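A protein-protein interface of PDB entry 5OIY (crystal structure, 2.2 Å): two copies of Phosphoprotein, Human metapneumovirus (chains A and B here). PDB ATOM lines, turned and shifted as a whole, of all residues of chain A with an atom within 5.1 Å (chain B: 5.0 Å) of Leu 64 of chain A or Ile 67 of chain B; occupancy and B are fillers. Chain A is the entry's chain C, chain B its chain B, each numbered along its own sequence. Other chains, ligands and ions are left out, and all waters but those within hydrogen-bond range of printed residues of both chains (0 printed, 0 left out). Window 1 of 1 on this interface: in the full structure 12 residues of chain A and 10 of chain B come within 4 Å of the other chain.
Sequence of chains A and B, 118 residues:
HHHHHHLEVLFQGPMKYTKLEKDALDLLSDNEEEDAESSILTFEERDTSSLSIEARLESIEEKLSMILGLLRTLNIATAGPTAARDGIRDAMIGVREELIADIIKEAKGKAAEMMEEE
Ile 60 of chain A touches Ile 60 of chain B (CG2 to CD1, 3.7 Å).
CD1 of Ile 60 of chain B touches CG of Glu 61 of chain A, 3.8 Å away.
CD1 of Leu 64 of chain A touches CG2 of Ile 60 of chain B (3.5 Å).
Leu 64 of chain B touches Leu 64 of chain A.
CD2 of Leu 64 of chain A touches CD1 of Ile 67 of chain B, 3.9 Å away.
Ile 67 of chain B touches Ile 67 of chain A (CD1 to CG2, 3.6 Å).
CD2 of Leu 68 of chain A touches CB of Met 66 of chain B (3.8 Å).
CD2 of Leu 68 of chain A touches CG1 of Ile 67 of chain B, at 3.5 Å.
Leu 68 of chain A touches Leu 70 of chain B.
Leu 71 of chain A touches Leu 70 of chain B (CB to CD1, 3.5 Å).
Of chain B, only Ile 60 (3.5 Å), Leu 64 (3.7 Å) and Ile 67 (3.9 Å) come within 4 Å of Leu 64 of chain A.
Printed residues of chain A within 4 Å of Ile 67 of chain B: Leu 64 (3.9 Å), Ile 67 (3.6 Å), Leu 68 (3.5 Å) and Leu 71 (3.8 Å).
Printed residues of chain A within 4 Å of Leu 64 of chain B: Leu 64 (3.7 Å).
Printed residues of chain A within 4 Å of Lys 63 of chain B: Leu 68.
Leu 71 of chain B touches none of the printed residues of chain A.
The nearest printed residue of chain B that does not touch Glu 61 of chain A is Lys 63 of chain B (5.3 Å).
Of the 11 printed residues of chain A, 6 touch a printed residue of chain B.
Printed residues of chain A that touch a printed residue of chain B: Ile 60, Glu 61, Leu 64, Ile 67, Leu 68 and Leu 71.
Along chain A the printed residues that touch a printed residue of chain B span positions 60 to 71.
Of the 10 printed residues of chain B, 6 touch a printed residue of chain A.
Hydrophobic or aromatic side chains of chain B within 4 Å of the printed part of chain A: Ile 60, Leu 64, Met 66, Ile 67 and Leu 70.
Among the printed residues, 12 pairs touch across the chains.
Among the printed residues, no Asp or Glu carboxylate lies within 4 Å of a Lys or Arg side-chain nitrogen of the other chain.
Leu 64 of chain A touches Ile 60 of chain B, but with the chains exchanged Ile 60 of chain A does not touch Leu 64 of chain B (6.9 Å).
Leu 64 of chain B touches its own counterpart, Leu 64 of chain A.
Ile 67 of chain A touches its own counterpart, Ile 67 of chain B.
Leu 68 of chain A touches Lys 63 of chain B, but with the chains exchanged Lys 63 of chain A does not touch Leu 68 of chain B (11.4 Å).
Of the 12 pairs that touch across the chains among the printed residues, 3 have their exchanged pair printed and touching as well.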
ATOM      1  N   ILE A  60      28.844  27.764 -10.364  1.00  0.00           N
ATOM      2  CA  ILE A  60      27.576  27.948  -9.659  1.00  0.00           C
ATOM      3  C   ILE A  60      27.404  26.903  -8.560  1.00  0.00           C
ATOM      4  O   ILE A  60      27.114  27.239  -7.416  1.00  0.00           O
ATOM      5  CB  ILE A  60      26.387  27.849 -10.626  1.00  0.00           C
ATOM      6  CG1 ILE A  60      26.249  29.139 -11.431  1.00  0.00           C
ATOM      7  CG2 ILE A  60      25.109  27.543  -9.868  1.00  0.00           C
ATOM      8  CD1 ILE A  60      25.491  28.972 -12.727  1.00  0.00           C
ATOM      9  N   GLU A  61      27.587  25.635  -8.905  1.00  0.00           N
ATOM     10  CA  GLU A  61      27.488  24.566  -7.924  1.00  0.00           C
ATOM     11  C   GLU A  61      28.504  24.743  -6.796  1.00  0.00           C
ATOM     12  O   GLU A  61      28.184  24.422  -5.654  1.00  0.00           O
ATOM     13  CB  GLU A  61      27.726  23.221  -8.583  1.00  0.00           C
ATOM     14  CG  GLU A  61      26.760  22.914  -9.700  1.00  0.00           C
ATOM     15  CD  GLU A  61      27.230  21.760 -10.550  1.00  0.00           C
ATOM     16  OE1 GLU A  61      28.435  21.707 -10.864  1.00  0.00           O
ATOM     17  OE2 GLU A  61      26.390  20.914 -10.906  1.00  0.00           O
ATOM     18  N   GLU A  62      29.732  25.167  -7.109  1.00  0.00           N
ATOM     19  CA  GLU A  62      30.720  25.437  -6.094  1.00  0.00           C
ATOM     20  C   GLU A  62      30.141  26.384  -5.052  1.00  0.00           C
ATOM     21  O   GLU A  62      30.058  26.018  -3.881  1.00  0.00           O
ATOM     22  CB  GLU A  62      31.978  26.041  -6.722  1.00  0.00           C
ATOM     23  CG  GLU A  62      32.977  26.578  -5.716  1.00  0.00           C
ATOM     24  CD  GLU A  62      33.534  25.498  -4.807  1.00  0.00           C
ATOM     25  OE1 GLU A  62      34.105  24.517  -5.327  1.00  0.00           O
ATOM     26  OE2 GLU A  62      33.407  25.633  -3.570  1.00  0.00           O
ATOM     27  N   LYS A  63      29.750  27.627  -5.437  1.00  0.00           N
ATOM     28  CA  LYS A  63      29.182  28.655  -4.583  1.00  0.00           C
ATOM     29  C   LYS A  63      27.968  28.168  -3.773  1.00  0.00           C
ATOM     30  O   LYS A  63      27.861  28.493  -2.600  1.00  0.00           O
ATOM     31  CB  LYS A  63      28.796  29.862  -5.427  1.00  0.00           C
ATOM     32  CG  LYS A  63      29.964  30.518  -6.139  1.00  0.00           C
ATOM     33  CD  LYS A  63      29.481  31.545  -7.151  1.00  0.00           C
ATOM     34  CE  LYS A  63      30.550  32.571  -7.482  1.00  0.00           C
ATOM     35  NZ  LYS A  63      31.681  31.996  -8.261  1.00  0.00           N
ATOM     36  N   LEU A  64      27.064  27.393  -4.365  1.00  0.00           N
ATOM     37  CA  LEU A  64      25.915  26.904  -3.610  1.00  0.00           C
ATOM     38  C   LEU A  64      26.318  26.012  -2.439  1.00  0.00           C
ATOM     39  O   LEU A  64      25.776  26.156  -1.351  1.00  0.00           O
ATOM     40  CB  LEU A  64      24.966  26.139  -4.515  1.00  0.00           C
ATOM     41  CG  LEU A  64      24.269  27.000  -5.557  1.00  0.00           C
ATOM     42  CD1 LEU A  64      23.487  26.110  -6.497  1.00  0.00           C
ATOM     43  CD2 LEU A  64      23.364  28.021  -4.890  1.00  0.00           C
ATOM     44  N   SER A  65      27.253  25.089  -2.650  1.00  0.00           N
ATOM     45  CA  SER A  65      27.738  24.262  -1.547  1.00  0.00           C
ATOM     46  C   SER A  65      28.413  25.145  -0.476  1.00  0.00           C
ATOM     47  O   SER A  65      28.233  24.899   0.711  1.00  0.00           O
ATOM     48  CB  SER A  65      28.690  23.168  -2.041  1.00  0.00           C
ATOM     49  OG  SER A  65      29.861  23.716  -2.612  1.00  0.00           O
ATOM     50  N   MET A  66      29.191  26.153  -0.880  1.00  0.00           N
ATOM     51  CA  MET A  66      29.799  27.066   0.060  1.00  0.00           C
ATOM     52  C   MET A  66      28.707  27.796   0.865  1.00  0.00           C
ATOM     53  O   MET A  66      28.806  27.875   2.086  1.00  0.00           O
ATOM     54  CB  MET A  66      30.626  28.074  -0.748  1.00  0.00           C
ATOM     55  CG  MET A  66      31.862  28.642  -0.075  1.00  0.00           C
ATOM     56  SD  MET A  66      32.886  29.495  -1.295  1.00  0.00           S
ATOM     57  CE  MET A  66      34.455  29.595  -0.444  1.00  0.00           C
ATOM     58  N   ILE A  67      27.663  28.311   0.207  1.00  0.00           N
ATOM     59  CA  ILE A  67      26.564  28.964   0.911  1.00  0.00           C
ATOM     60  C   ILE A  67      25.770  28.000   1.804  1.00  0.00           C
ATOM     61  O   ILE A  67      25.474  28.327   2.945  1.00  0.00           O
ATOM     62  CB  ILE A  67      25.614  29.667  -0.078  1.00  0.00           C
ATOM     63  CG1 ILE A  67      26.340  30.809  -0.782  1.00  0.00           C
ATOM     64  CG2 ILE A  67      24.393  30.208   0.641  1.00  0.00           C
ATOM     65  CD1 ILE A  67      25.650  31.291  -2.038  1.00  0.00           C
ATOM     66  N   LEU A  68      25.451  26.807   1.306  1.00  0.00           N
ATOM     67  CA  LEU A  68      24.727  25.824   2.103  1.00  0.00           C
ATOM     68  C   LEU A  68      25.499  25.383   3.348  1.00  0.00           C
ATOM     69  O   LEU A  68      24.899  25.205   4.405  1.00  0.00           O
ATOM     70  CB  LEU A  68      24.396  24.595   1.265  1.00  0.00           C
ATOM     71  CG  LEU A  68      22.963  24.491   0.758  1.00  0.00           C
ATOM     72  CD1 LEU A  68      22.711  23.104   0.189  1.00  0.00           C
ATOM     73  CD2 LEU A  68      21.979  24.792   1.876  1.00  0.00           C
ATOM     74  N   GLY A  69      26.810  25.164   3.232  1.00  0.00           N
ATOM     75  CA  GLY A  69      27.611  24.800   4.382  1.00  0.00           C
ATOM     76  C   GLY A  69      27.634  25.877   5.457  1.00  0.00           C
ATOM     77  O   GLY A  69      27.532  25.555   6.637  1.00  0.00           O
ATOM     78  N   LEU A  71      25.322  28.209   6.195  1.00  0.00           N
ATOM     79  CA  LEU A  71      24.064  28.293   6.891  1.00  0.00           C
ATOM     80  C   LEU A  71      23.847  27.140   7.860  1.00  0.00           C
ATOM     81  O   LEU A  71      23.499  27.384   9.010  1.00  0.00           O
ATOM     82  CB  LEU A  71      22.911  28.384   5.893  1.00  0.00           C
ATOM     83  CG  LEU A  71      23.021  29.549   4.909  1.00  0.00           C
ATOM     84  CD1 LEU A  71      21.760  29.658   4.075  1.00  0.00           C
ATOM     85  CD2 LEU A  71      23.289  30.856   5.631  1.00  0.00           C
ATOM     86  N   ILE B  60      20.965  21.910  -8.484  1.00  0.00           N
ATOM     87  CA  ILE B  60      21.129  23.309  -8.133  1.00  0.00           C
ATOM     88  C   ILE B  60      19.800  23.887  -7.632  1.00  0.00           C
ATOM     89  O   ILE B  60      19.794  24.641  -6.666  1.00  0.00           O
ATOM     90  CB  ILE B  60      21.591  24.124  -9.350  1.00  0.00           C
ATOM     91  CG1 ILE B  60      23.083  23.922  -9.592  1.00  0.00           C
ATOM     92  CG2 ILE B  60      21.290  25.598  -9.166  1.00  0.00           C
ATOM     93  CD1 ILE B  60      23.524  24.333 -10.975  1.00  0.00           C
ATOM     94  N   LYS B  63      19.273  22.693  -3.912  1.00  0.00           N
ATOM     95  CA  LYS B  63      20.105  23.422  -2.972  1.00  0.00           C
ATOM     96  C   LYS B  63      19.566  24.835  -2.750  1.00  0.00           C
ATOM     97  O   LYS B  63      19.612  25.327  -1.626  1.00  0.00           O
ATOM     98  CB  LYS B  63      21.548  23.472  -3.459  1.00  0.00           C
ATOM     99  CG  LYS B  63      22.246  22.129  -3.365  1.00  0.00           C
ATOM    100  CD  LYS B  63      23.717  22.228  -3.710  1.00  0.00           C
ATOM    101  CE  LYS B  63      24.403  20.890  -3.499  1.00  0.00           C
ATOM    102  NZ  LYS B  63      23.685  19.802  -4.211  1.00  0.00           N
ATOM    103  N   LEU B  64      19.104  25.513  -3.801  1.00  0.00           N
ATOM    104  CA  LEU B  64      18.519  26.816  -3.616  1.00  0.00           C
ATOM    105  C   LEU B  64      17.362  26.737  -2.629  1.00  0.00           C
ATOM    106  O   LEU B  64      17.279  27.596  -1.762  1.00  0.00           O
ATOM    107  CB  LEU B  64      18.086  27.427  -4.945  1.00  0.00           C
ATOM    108  CG  LEU B  64      19.257  28.003  -5.739  1.00  0.00           C
ATOM    109  CD1 LEU B  64      18.833  28.329  -7.155  1.00  0.00           C
ATOM    110  CD2 LEU B  64      19.848  29.226  -5.060  1.00  0.00           C
ATOM    111  N   SER B  65      16.398  25.768  -2.752  1.00  0.00           N
ATOM    112  CA  SER B  65      15.278  25.592  -1.833  1.00  0.00           C
ATOM    113  C   SER B  65      15.767  25.434  -0.388  1.00  0.00           C
ATOM    114  O   SER B  65      15.208  26.050   0.515  1.00  0.00           O
ATOM    115  CB  SER B  65      14.477  24.351  -2.213  1.00  0.00           C
ATOM    116  OG  SER B  65      13.660  24.596  -3.337  1.00  0.00           O
ATOM    117  N   MET B  66      16.776  24.590  -0.166  1.00  0.00           N
ATOM    118  CA  MET B  66      17.372  24.431   1.158  1.00  0.00           C
ATOM    119  C   MET B  66      17.917  25.757   1.693  1.00  0.00           C
ATOM    120  O   MET B  66      17.700  26.084   2.854  1.00  0.00           O
ATOM    121  CB  MET B  66      18.501  23.408   1.112  1.00  0.00           C
ATOM    122  CG  MET B  66      18.031  21.974   0.994  1.00  0.00           C
ATOM    123  SD  MET B  66      19.336  20.881   0.411  1.00  0.00           S
ATOM    124  CE  MET B  66      18.495  19.305   0.478  1.00  0.00           C
ATOM    125  N   ILE B  67      18.639  26.511   0.868  1.00  0.00           N
ATOM    126  CA  ILE B  67      19.162  27.802   1.289  1.00  0.00           C
ATOM    127  C   ILE B  67      18.048  28.786   1.671  1.00  0.00           C
ATOM    128  O   ILE B  67      18.176  29.492   2.665  1.00  0.00           O
ATOM    129  CB  ILE B  67      20.019  28.423   0.177  1.00  0.00           C
ATOM    130  CG1 ILE B  67      21.273  27.583  -0.038  1.00  0.00           C
ATOM    131  CG2 ILE B  67      20.390  29.856   0.511  1.00  0.00           C
ATOM    132  CD1 ILE B  67      22.135  28.056  -1.183  1.00  0.00           C
ATOM    133  N   LEU B  68      16.965  28.846   0.899  1.00  0.00           N
ATOM    134  CA  LEU B  68      15.859  29.723   1.246  1.00  0.00           C
ATOM    135  C   LEU B  68      15.224  29.328   2.591  1.00  0.00           C
ATOM    136  O   LEU B  68      14.925  30.197   3.402  1.00  0.00           O
ATOM    137  CB  LEU B  68      14.807  29.709   0.141  1.00  0.00           C
ATOM    138  CG  LEU B  68      13.759  30.814   0.241  1.00  0.00           C
ATOM    139  CD1 LEU B  68      14.419  32.176   0.366  1.00  0.00           C
ATOM    140  CD2 LEU B  68      12.828  30.775  -0.957  1.00  0.00           C
ATOM    141  N   GLY B  69      15.018  28.037   2.840  1.00  0.00           N
ATOM    142  CA  GLY B  69      14.481  27.616   4.118  1.00  0.00           C
ATOM    143  C   GLY B  69      15.391  27.977   5.287  1.00  0.00           C
ATOM    144  O   GLY B  69      14.906  28.462   6.304  1.00  0.00           O
ATOM    145  N   LEU B  70      16.700  27.763   5.158  1.00  0.00           N
ATOM    146  CA  LEU B  70      17.631  28.123   6.220  1.00  0.00           C
ATOM    147  C   LEU B  70      17.672  29.626   6.511  1.00  0.00           C
ATOM    148  O   LEU B  70      17.707  30.017   7.673  1.00  0.00           O
ATOM    149  CB  LEU B  70      19.035  27.636   5.878  1.00  0.00           C
ATOM    150  CG  LEU B  70      19.181  26.120   5.787  1.00  0.00           C
ATOM    151  CD1 LEU B  70      20.585  25.760   5.340  1.00  0.00           C
ATOM    152  CD2 LEU B  70      18.852  25.468   7.117  1.00  0.00           C
ATOM    153  N   LEU B  71      17.675  30.468   5.481  1.00  0.00           N
ATOM    154  CA  LEU B  71      17.677  31.912   5.688  1.00  0.00           C
ATOM    155  C   LEU B  71      16.441  32.417   6.426  1.00  0.00           C
ATOM    156  O   LEU B  71      16.550  33.262   7.303  1.00  0.00           O
ATOM    157  CB  LEU B  71      17.748  32.632   4.352  1.00  0.00           C
ATOM    158  CG  LEU B  71      19.137  32.835   3.775  1.00  0.00           C
ATOM    159  CD1 LEU B  71      19.009  33.535   2.439  1.00  0.00           C
ATOM    160  CD2 LEU B  71      19.996  33.642   4.729  1.00  0.00           C
